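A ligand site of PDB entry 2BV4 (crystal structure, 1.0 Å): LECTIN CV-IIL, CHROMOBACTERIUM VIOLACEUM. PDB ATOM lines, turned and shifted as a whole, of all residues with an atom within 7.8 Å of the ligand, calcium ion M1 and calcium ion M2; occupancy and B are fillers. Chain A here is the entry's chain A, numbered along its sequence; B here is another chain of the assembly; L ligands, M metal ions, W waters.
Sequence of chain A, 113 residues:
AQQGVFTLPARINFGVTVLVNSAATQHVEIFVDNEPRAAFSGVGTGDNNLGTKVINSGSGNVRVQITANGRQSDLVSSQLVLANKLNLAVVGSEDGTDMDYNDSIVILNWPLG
Calcium ion M2 is bound by OD1 of Asn 102 (2.3 Å), O of Asn 21 (2.3 Å), OD1 of Asp 103 (2.4 Å), O of Gly 113 of chain B (2.4 Å), OD2 of Asp 100 (2.4 Å), O3 of the ligand (2.5 Å) and O2 of the ligand (2.5 Å).
Slightly farther from calcium ion M2 lies OD1 of Asp 100 (3.0 Å).
Four residues have an atom within 4 Å of calcium ion M1: Glu 94, Asp 98, Asp 100 and Asp 103.
N of Asn 102 sits at hydrogen-bond distance from O of Ser 93, 3.4 Å away.
The backbone NH (N) of Asn 21 lies close to the backbone carbonyl oxygen (O) of Gly 44 (3.4 Å).
The backbone NH of Gly 113 of chain B sits close to the backbone carbonyl oxygen of Thr 45 (3.3 Å).
OE2 of Glu 94 sits close to N of Gly 96 (2.8 Å).
OD2 of Asp 95 sits at hydrogen-bond distance from OG of Ser 22, at 2.7 Å.
The side-chain carboxylate (OD2) of Asp 95 lies within hydrogen-bond range of the side-chain amide nitrogen (NE2) of Gln 26, 2.9 Å away.
N of Ala 24 is in hydrogen-bond range of OG of Ser 22, at 3.0 Å.
N of Ser 22 sits at hydrogen-bond distance from O of Gly 44 (2.8 Å).
Merely in contact with the ligand: Ser 22 (3.2 Å) and Ala 24 (3.9 Å).
Hydrophobic or aromatic side chains within 4 Å of the ligand: Ala 23.
Within 4 Å of the ligand: Asn 21, Ser 22, Ala 23, Ala 24, Glu 94, Asp 95, Asp 98, Asp 100, Asp 103 and Gly 113 of chain B.
Along chain A the residues within 4 Å of the ligand span positions 21 to 103.
Calcium ion M1 is bound by the side-chain carboxylate (OD1) of Asp 100, the side-chain carboxylate (OD1) of Asp 98, the side-chain carboxylate (OE2) of Glu 94, the side-chain carboxylate (OD2) of Asp 103, the side-chain carboxylate (OE1) of Glu 94, an oxygen (O3) of the ligand, an oxygen (O4) of the ligand and the side-chain carboxylate (OD1) of Asp 103.
The side-chain carboxylate (OD1) of Asp 95 lies close to an oxygen (O4) of the ligand (2.6 Å).
The backbone NH (N) of Ala 23 lies within hydrogen-bond range of an oxygen (O5) of the ligand.
Water W3 lies within hydrogen-bond range of an oxygen (O6) of the ligand and the side-chain amide nitrogen of Asn 69.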
ATOM      1  N   VAL A  20      25.603 -31.773   2.555  1.00  0.00           N
ATOM      2  CA  VAL A  20      24.313 -31.145   2.686  1.00  0.00           C
ATOM      3  C   VAL A  20      23.775 -31.223   4.123  1.00  0.00           C
ATOM      4  O   VAL A  20      24.012 -32.169   4.862  1.00  0.00           O
ATOM      5  CB  VAL A  20      23.280 -31.691   1.670  1.00  0.00           C
ATOM      6  CG1 VAL A  20      23.763 -31.428   0.232  1.00  0.00           C
ATOM      7  CG2 VAL A  20      22.954 -33.172   1.881  1.00  0.00           C
ATOM      8  N   ASN A  21      23.012 -30.179   4.455  1.00  0.00           N
ATOM      9  CA  ASN A  21      22.324 -30.077   5.746  1.00  0.00           C
ATOM     10  C   ASN A  21      21.012 -29.375   5.529  1.00  0.00           C
ATOM     11  O   ASN A  21      20.859 -28.189   5.887  1.00  0.00           O
ATOM     12  CB  ASN A  21      23.142 -29.300   6.791  1.00  0.00           C
ATOM     13  CG  ASN A  21      24.409 -30.001   7.178  1.00  0.00           C
ATOM     14  OD1 ASN A  21      24.428 -30.835   8.095  1.00  0.00           O
ATOM     15  ND2 ASN A  21      25.518 -29.632   6.515  1.00  0.00           N
ATOM     16  N   SER A  22      20.079 -30.030   4.855  1.00  0.00           N
ATOM     17  CA  SER A  22      18.836 -29.379   4.453  1.00  0.00           C
ATOM     18  C   SER A  22      17.745 -30.407   4.242  1.00  0.00           C
ATOM     19  O   SER A  22      17.989 -31.529   3.814  1.00  0.00           O
ATOM     20  CB  SER A  22      19.032 -28.666   3.106  1.00  0.00           C
ATOM     21  OG  SER A  22      17.782 -27.811   2.937  1.00  0.00           O
ATOM     22  N   ALA A  23      16.501 -29.987   4.470  1.00  0.00           N
ATOM     23  CA  ALA A  23      15.329 -30.746   4.090  1.00  0.00           C
ATOM     24  C   ALA A  23      14.964 -30.578   2.614  1.00  0.00           C
ATOM     25  O   ALA A  23      14.174 -31.372   2.086  1.00  0.00           O
ATOM     26  CB  ALA A  23      14.134 -30.320   4.975  1.00  0.00           C
ATOM     27  N   ALA A  24      15.497 -29.547   1.950  1.00  0.00           N
ATOM     28  CA  ALA A  24      15.260 -29.305   0.551  1.00  0.00           C
ATOM     29  C   ALA A  24      16.367 -29.956  -0.266  1.00  0.00           C
ATOM     30  O   ALA A  24      17.540 -29.891   0.096  1.00  0.00           O
ATOM     31  CB  ALA A  24      15.234 -27.832   0.250  1.00  0.00           C
ATOM     32  N   THR A  25      16.009 -30.570  -1.387  1.00  0.00           N
ATOM     33  CA  THR A  25      17.028 -31.129  -2.254  1.00  0.00           C
ATOM     34  C   THR A  25      17.900 -30.012  -2.806  1.00  0.00           C
ATOM     35  O   THR A  25      17.433 -28.984  -3.286  1.00  0.00           O
ATOM     36  CB  THR A  25      16.363 -31.923  -3.400  1.00  0.00           C
ATOM     37  OG1 THR A  25      15.589 -32.962  -2.799  1.00  0.00           O
ATOM     38  CG2 THR A  25      17.381 -32.526  -4.318  1.00  0.00           C
ATOM     39  N   GLN A  26      19.192 -30.257  -2.763  1.00  0.00           N
ATOM     40  CA  GLN A  26      20.259 -29.329  -3.191  1.00  0.00           C
ATOM     41  C   GLN A  26      20.768 -29.745  -4.541  1.00  0.00           C
ATOM     42  O   GLN A  26      20.944 -30.945  -4.796  1.00  0.00           O
ATOM     43  CB  GLN A  26      21.417 -29.365  -2.184  1.00  0.00           C
ATOM     44  CG  GLN A  26      21.007 -29.109  -0.738  1.00  0.00           C
ATOM     45  CD  GLN A  26      20.549 -27.697  -0.503  1.00  0.00           C
ATOM     46  OE1 GLN A  26      21.320 -26.748  -0.714  1.00  0.00           O
ATOM     47  NE2 GLN A  26      19.309 -27.538  -0.045  1.00  0.00           N
ATOM     48  N   VAL A  43      19.979 -34.656  -0.615  1.00  0.00           N
ATOM     49  CA  VAL A  43      19.162 -34.072   0.434  1.00  0.00           C
ATOM     50  C   VAL A  43      19.446 -34.808   1.732  1.00  0.00           C
ATOM     51  O   VAL A  43      19.700 -36.023   1.713  1.00  0.00           O
ATOM     52  CB  VAL A  43      17.665 -34.148   0.077  1.00  0.00           C
ATOM     53  CG1 VAL A  43      17.147 -35.573  -0.064  1.00  0.00           C
ATOM     54  CG2 VAL A  43      16.819 -33.362   1.060  1.00  0.00           C
ATOM     55  N   GLY A  44      19.397 -34.118   2.844  1.00  0.00           N
ATOM     56  CA  GLY A  44      19.595 -34.718   4.143  1.00  0.00           C
ATOM     57  C   GLY A  44      20.105 -33.691   5.123  1.00  0.00           C
ATOM     58  O   GLY A  44      20.779 -32.714   4.736  1.00  0.00           O
ATOM     59  N   THR A  45      19.813 -33.896   6.408  1.00  0.00           N
ATOM     60  CA  THR A  45      20.146 -32.946   7.445  1.00  0.00           C
ATOM     61  C   THR A  45      21.331 -33.389   8.302  1.00  0.00           C
ATOM     62  O   THR A  45      21.660 -32.717   9.299  1.00  0.00           O
ATOM     63  CB  THR A  45      18.938 -32.670   8.319  1.00  0.00           C
ATOM     64  OG1 THR A  45      18.419 -33.877   8.850  1.00  0.00           O
ATOM     65  CG2 THR A  45      17.835 -31.960   7.542  1.00  0.00           C
ATOM     66  N   ALA A  68      18.132 -24.633  -4.809  1.00  0.00           N
ATOM     67  CA  ALA A  68      17.174 -25.459  -4.048  1.00  0.00           C
ATOM     68  C   ALA A  68      15.819 -24.804  -4.260  1.00  0.00           C
ATOM     69  O   ALA A  68      15.720 -23.570  -4.313  1.00  0.00           O
ATOM     70  CB  ALA A  68      17.535 -25.546  -2.567  1.00  0.00           C
ATOM     71  N   ASN A  69      14.757 -25.622  -4.390  1.00  0.00           N
ATOM     72  CA  ASN A  69      13.413 -25.083  -4.651  1.00  0.00           C
ATOM     73  C   ASN A  69      13.389 -24.172  -5.860  1.00  0.00           C
ATOM     74  O   ASN A  69      12.576 -23.255  -5.933  1.00  0.00           O
ATOM     75  CB  ASN A  69      12.852 -24.365  -3.428  1.00  0.00           C
ATOM     76  CG  ASN A  69      12.788 -25.241  -2.218  1.00  0.00           C
ATOM     77  OD1 ASN A  69      12.134 -26.291  -2.227  1.00  0.00           O
ATOM     78  ND2 ASN A  69      13.470 -24.834  -1.132  1.00  0.00           N
ATOM     79  N   SER A  93      25.951 -21.918   2.072  1.00  0.00           N
ATOM     80  CA  SER A  93      24.759 -21.443   1.362  1.00  0.00           C
ATOM     81  C   SER A  93      23.537 -21.606   2.200  1.00  0.00           C
ATOM     82  O   SER A  93      23.434 -22.485   3.057  1.00  0.00           O
ATOM     83  CB  SER A  93      24.616 -22.209   0.058  1.00  0.00           C
ATOM     84  OG  SER A  93      24.347 -23.600   0.250  1.00  0.00           O
ATOM     85  N   GLU A  94      22.585 -20.706   1.934  1.00  0.00           N
ATOM     86  CA  GLU A  94      21.327 -20.641   2.659  1.00  0.00           C
ATOM     87  C   GLU A  94      20.174 -20.675   1.649  1.00  0.00           C
ATOM     88  O   GLU A  94      20.044 -19.800   0.779  1.00  0.00           O
ATOM     89  CB  GLU A  94      21.264 -19.361   3.510  1.00  0.00           C
ATOM     90  CG  GLU A  94      19.961 -19.216   4.275  1.00  0.00           C
ATOM     91  CD  GLU A  94      19.645 -20.423   5.111  1.00  0.00           C
ATOM     92  OE1 GLU A  94      20.499 -20.895   5.876  1.00  0.00           O
ATOM     93  OE2 GLU A  94      18.505 -20.976   4.997  1.00  0.00           O
ATOM     94  N   ASP A  95      19.321 -21.664   1.811  1.00  0.00           N
ATOM     95  CA  ASP A  95      18.190 -21.919   0.941  1.00  0.00           C
ATOM     96  C   ASP A  95      16.868 -21.450   1.542  1.00  0.00           C
ATOM     97  O   ASP A  95      15.809 -21.615   0.879  1.00  0.00           O
ATOM     98  CB  ASP A  95      18.092 -23.399   0.555  1.00  0.00           C
ATOM     99  CG  ASP A  95      17.786 -24.315   1.720  1.00  0.00           C
ATOM    100  OD1 ASP A  95      17.161 -23.836   2.704  1.00  0.00           O
ATOM    101  OD2 ASP A  95      18.097 -25.530   1.594  1.00  0.00           O
ATOM    102  N   GLY A  96      16.881 -20.873   2.723  1.00  0.00           N
ATOM    103  CA  GLY A  96      15.668 -20.653   3.487  1.00  0.00           C
ATOM    104  C   GLY A  96      15.776 -19.472   4.400  1.00  0.00           C
ATOM    105  O   GLY A  96      16.316 -18.428   4.025  1.00  0.00           O
ATOM    106  N   THR A  97      15.234 -19.642   5.608  1.00  0.00           N
ATOM    107  CA  THR A  97      14.987 -18.544   6.547  1.00  0.00           C
ATOM    108  C   THR A  97      15.763 -18.603   7.835  1.00  0.00           C
ATOM    109  O   THR A  97      15.709 -17.647   8.614  1.00  0.00           O
ATOM    110  CB  THR A  97      13.488 -18.486   6.888  1.00  0.00           C
ATOM    111  OG1 THR A  97      13.118 -19.732   7.496  1.00  0.00           O
ATOM    112  CG2 THR A  97      12.673 -18.312   5.659  1.00  0.00           C
ATOM    113  N   ASP A  98      16.464 -19.703   8.138  1.00  0.00           N
ATOM    114  CA  ASP A  98      17.095 -19.863   9.417  1.00  0.00           C
ATOM    115  C   ASP A  98      18.541 -19.382   9.475  1.00  0.00           C
ATOM    116  O   ASP A  98      19.149 -19.433  10.545  1.00  0.00           O
ATOM    117  CB  ASP A  98      16.983 -21.323   9.918  1.00  0.00           C
ATOM    118  CG  ASP A  98      17.768 -22.296   9.090  1.00  0.00           C
ATOM    119  OD1 ASP A  98      18.242 -21.963   7.985  1.00  0.00           O
ATOM    120  OD2 ASP A  98      17.909 -23.453   9.552  1.00  0.00           O
ATOM    121  N   MET A  99      19.103 -18.933   8.360  1.00  0.00           N
ATOM    122  CA  MET A  99      20.450 -18.354   8.327  1.00  0.00           C
ATOM    123  C   MET A  99      21.499 -19.266   8.964  1.00  0.00           C
ATOM    124  O   MET A  99      22.432 -18.776   9.600  1.00  0.00           O
ATOM    125  CB  MET A  99      20.472 -16.964   8.983  1.00  0.00           C
ATOM    126  CG  MET A  99      19.544 -15.989   8.349  1.00  0.00           C
ATOM    127  SD  MET A  99      19.645 -14.334   9.027  1.00  0.00           S
ATOM    128  CE  MET A  99      18.192 -13.617   8.288  1.00  0.00           C
ATOM    129  N   ASP A 100      21.412 -20.583   8.726  1.00  0.00           N
ATOM    130  CA  ASP A 100      22.462 -21.501   9.168  1.00  0.00           C
ATOM    131  C   ASP A 100      23.599 -21.666   8.174  1.00  0.00           C
ATOM    132  O   ASP A 100      24.691 -22.093   8.548  1.00  0.00           O
ATOM    133  CB  ASP A 100      21.904 -22.819   9.724  1.00  0.00           C
ATOM    134  CG  ASP A 100      21.240 -23.752   8.714  1.00  0.00           C
ATOM    135  OD1 ASP A 100      21.050 -23.380   7.536  1.00  0.00           O
ATOM    136  OD2 ASP A 100      20.944 -24.889   9.144  1.00  0.00           O
ATOM    137  N   TYR A 101      23.370 -21.329   6.891  1.00  0.00           N
ATOM    138  CA  TYR A 101      24.417 -21.315   5.875  1.00  0.00           C
ATOM    139  C   TYR A 101      25.157 -22.632   5.711  1.00  0.00           C
ATOM    140  O   TYR A 101      26.264 -22.661   5.170  1.00  0.00           O
ATOM    141  CB  TYR A 101      25.390 -20.117   6.072  1.00  0.00           C
ATOM    142  CG  TYR A 101      24.727 -18.844   5.588  1.00  0.00           C
ATOM    143  CD1 TYR A 101      23.974 -18.064   6.415  1.00  0.00           C
ATOM    144  CD2 TYR A 101      24.806 -18.488   4.246  1.00  0.00           C
ATOM    145  CE1 TYR A 101      23.280 -16.956   5.888  1.00  0.00           C
ATOM    146  CE2 TYR A 101      24.111 -17.389   3.717  1.00  0.00           C
ATOM    147  CZ  TYR A 101      23.350 -16.660   4.547  1.00  0.00           C
ATOM    148  OH  TYR A 101      22.599 -15.578   4.100  1.00  0.00           O
ATOM    149  N   ASN A 102      24.472 -23.740   6.023  1.00  0.00           N
ATOM    150  CA  ASN A 102      25.072 -25.072   5.883  1.00  0.00           C
ATOM    151  C   ASN A 102      24.308 -25.942   4.905  1.00  0.00           C
ATOM    152  O   ASN A 102      24.551 -27.148   4.823  1.00  0.00           O
ATOM    153  CB  ASN A 102      25.186 -25.767   7.253  1.00  0.00           C
ATOM    154  CG  ASN A 102      23.825 -26.128   7.813  1.00  0.00           C
ATOM    155  OD1 ASN A 102      22.801 -25.958   7.121  1.00  0.00           O
ATOM    156  ND2 ASN A 102      23.770 -26.652   9.027  1.00  0.00           N
ATOM    157  N   ASP A 103      23.362 -25.357   4.168  1.00  0.00           N
ATOM    158  CA  ASP A 103      22.359 -26.188   3.474  1.00  0.00           C
ATOM    159  C   ASP A 103      23.022 -27.029   2.375  1.00  0.00           C
ATOM    160  O   ASP A 103      22.751 -28.229   2.252  1.00  0.00           O
ATOM    161  CB  ASP A 103      21.239 -25.306   2.944  1.00  0.00           C
ATOM    162  CG  ASP A 103      20.476 -24.613   4.066  1.00  0.00           C
ATOM    163  OD1 ASP A 103      20.282 -25.205   5.163  1.00  0.00           O
ATOM    164  OD2 ASP A 103      20.058 -23.455   3.888  1.00  0.00           O
ATOM    165  N   SER A 104      23.917 -26.402   1.619  1.00  0.00           N
ATOM    166  CA  SER A 104      25.037 -27.062   0.946  1.00  0.00           C
ATOM    167  C   SER A 104      26.316 -26.365   1.367  1.00  0.00           C
ATOM    168  O   SER A 104      26.367 -25.132   1.418  1.00  0.00           O
ATOM    169  CB  SER A 104      24.962 -26.998  -0.564  1.00  0.00           C
ATOM    170  OG  SER A 104      23.868 -27.722  -1.103  1.00  0.00           O
ATOM    171  N   LYS B  85      28.403 -17.925  11.421  1.00  0.00           N
ATOM    172  CA  LYS B  85      27.549 -19.089  11.693  1.00  0.00           C
ATOM    173  C   LYS B  85      28.184 -20.401  11.300  1.00  0.00           C
ATOM    174  O   LYS B  85      28.217 -21.352  12.099  1.00  0.00           O
ATOM    175  CB  LYS B  85      26.215 -18.904  10.946  1.00  0.00           C
ATOM    176  CG  LYS B  85      25.246 -20.011  11.148  1.00  0.00           C
ATOM    177  CD  LYS B  85      24.880 -20.111  12.597  1.00  0.00           C
ATOM    178  CE  LYS B  85      23.419 -20.434  12.820  1.00  0.00           C
ATOM    179  NZ  LYS B  85      23.145 -21.862  12.904  1.00  0.00           N
ATOM    180  N   PRO B 111      27.487 -25.670  12.899  1.00  0.00           N
ATOM    181  CA  PRO B 111      26.476 -26.648  13.296  1.00  0.00           C
ATOM    182  C   PRO B 111      25.912 -27.370  12.086  1.00  0.00           C
ATOM    183  O   PRO B 111      25.944 -26.875  10.949  1.00  0.00           O
ATOM    184  CB  PRO B 111      25.401 -25.780  13.978  1.00  0.00           C
ATOM    185  CG  PRO B 111      25.510 -24.464  13.257  1.00  0.00           C
ATOM    186  CD  PRO B 111      26.978 -24.284  12.967  1.00  0.00           C
ATOM    187  N   LEU B 112      25.318 -28.537  12.339  1.00  0.00           N
ATOM    188  CA  LEU B 112      24.661 -29.361  11.343  1.00  0.00           C
ATOM    189  C   LEU B 112      23.161 -29.074  11.316  1.00  0.00           C
ATOM    190  O   LEU B 112      22.650 -28.259  12.061  1.00  0.00           O
ATOM    191  CB  LEU B 112      24.952 -30.833  11.663  1.00  0.00           C
ATOM    192  CG  LEU B 112      26.445 -31.185  11.817  1.00  0.00           C
ATOM    193  CD1 LEU B 112      26.553 -32.682  12.023  1.00  0.00           C
ATOM    194  CD2 LEU B 112      27.240 -30.701  10.638  1.00  0.00           C
ATOM    195  N   GLY B 113      22.458 -29.781  10.454  1.00  0.00           N
ATOM    196  CA  GLY B 113      21.000 -29.802  10.444  1.00  0.00           C
ATOM    197  C   GLY B 113      20.357 -28.862   9.460  1.00  0.00           C
ATOM    198  O   GLY B 113      20.976 -27.870   8.988  1.00  0.00           O
ATOM    199  OXT GLY B 113      19.158 -29.147   9.179  1.00  0.00           O
HETATM  200  C1  LIG L   1      15.863 -27.528   7.300  1.00  0.00           C
HETATM  201  C2  LIG L   1      17.141 -26.891   7.794  1.00  0.00           C
HETATM  202  C3  LIG L   1      17.230 -25.473   7.243  1.00  0.00           C
HETATM  203  C4  LIG L   1      17.017 -25.470   5.721  1.00  0.00           C
HETATM  204  C5  LIG L   1      15.635 -26.099   5.444  1.00  0.00           C
HETATM  205  C6  LIG L   1      15.238 -26.213   3.982  1.00  0.00           C
HETATM  206  C7  LIG L   1      13.567 -27.674   7.803  1.00  0.00           C
HETATM  207  O1  LIG L   1      14.817 -27.022   8.033  1.00  0.00           O
HETATM  208  O2  LIG L   1      18.293 -27.579   7.331  1.00  0.00           O
HETATM  209  O3  LIG L   1      18.500 -24.892   7.546  1.00  0.00           O
HETATM  210  O4  LIG L   1      17.112 -24.109   5.293  1.00  0.00           O
HETATM  211  O5  LIG L   1      15.708 -27.465   5.918  1.00  0.00           O
HETATM  212  O6  LIG L   1      13.831 -26.560   3.969  1.00  0.00           O
HETATM  213 CA    CA M   1      19.237 -22.989   6.112  1.00  0.00          CA
HETATM  214 CA    CA M   2      20.489 -26.308   7.243  1.00  0.00          CA
HETATM  215  O   HOH W   1      12.104 -28.266   2.158  1.00  0.00           O
HETATM  216  O   HOH W   2      15.147 -22.400   6.539  1.00  0.00           O
HETATM  217  O   HOH W   3      12.781 -25.496   1.642  1.00  0.00           O
HETATM  218  O   HOH W   4      14.795 -24.944  10.387  1.00  0.00           O
HETATM  219  O   HOH W   5      11.923 -25.306   5.513  1.00  0.00           O
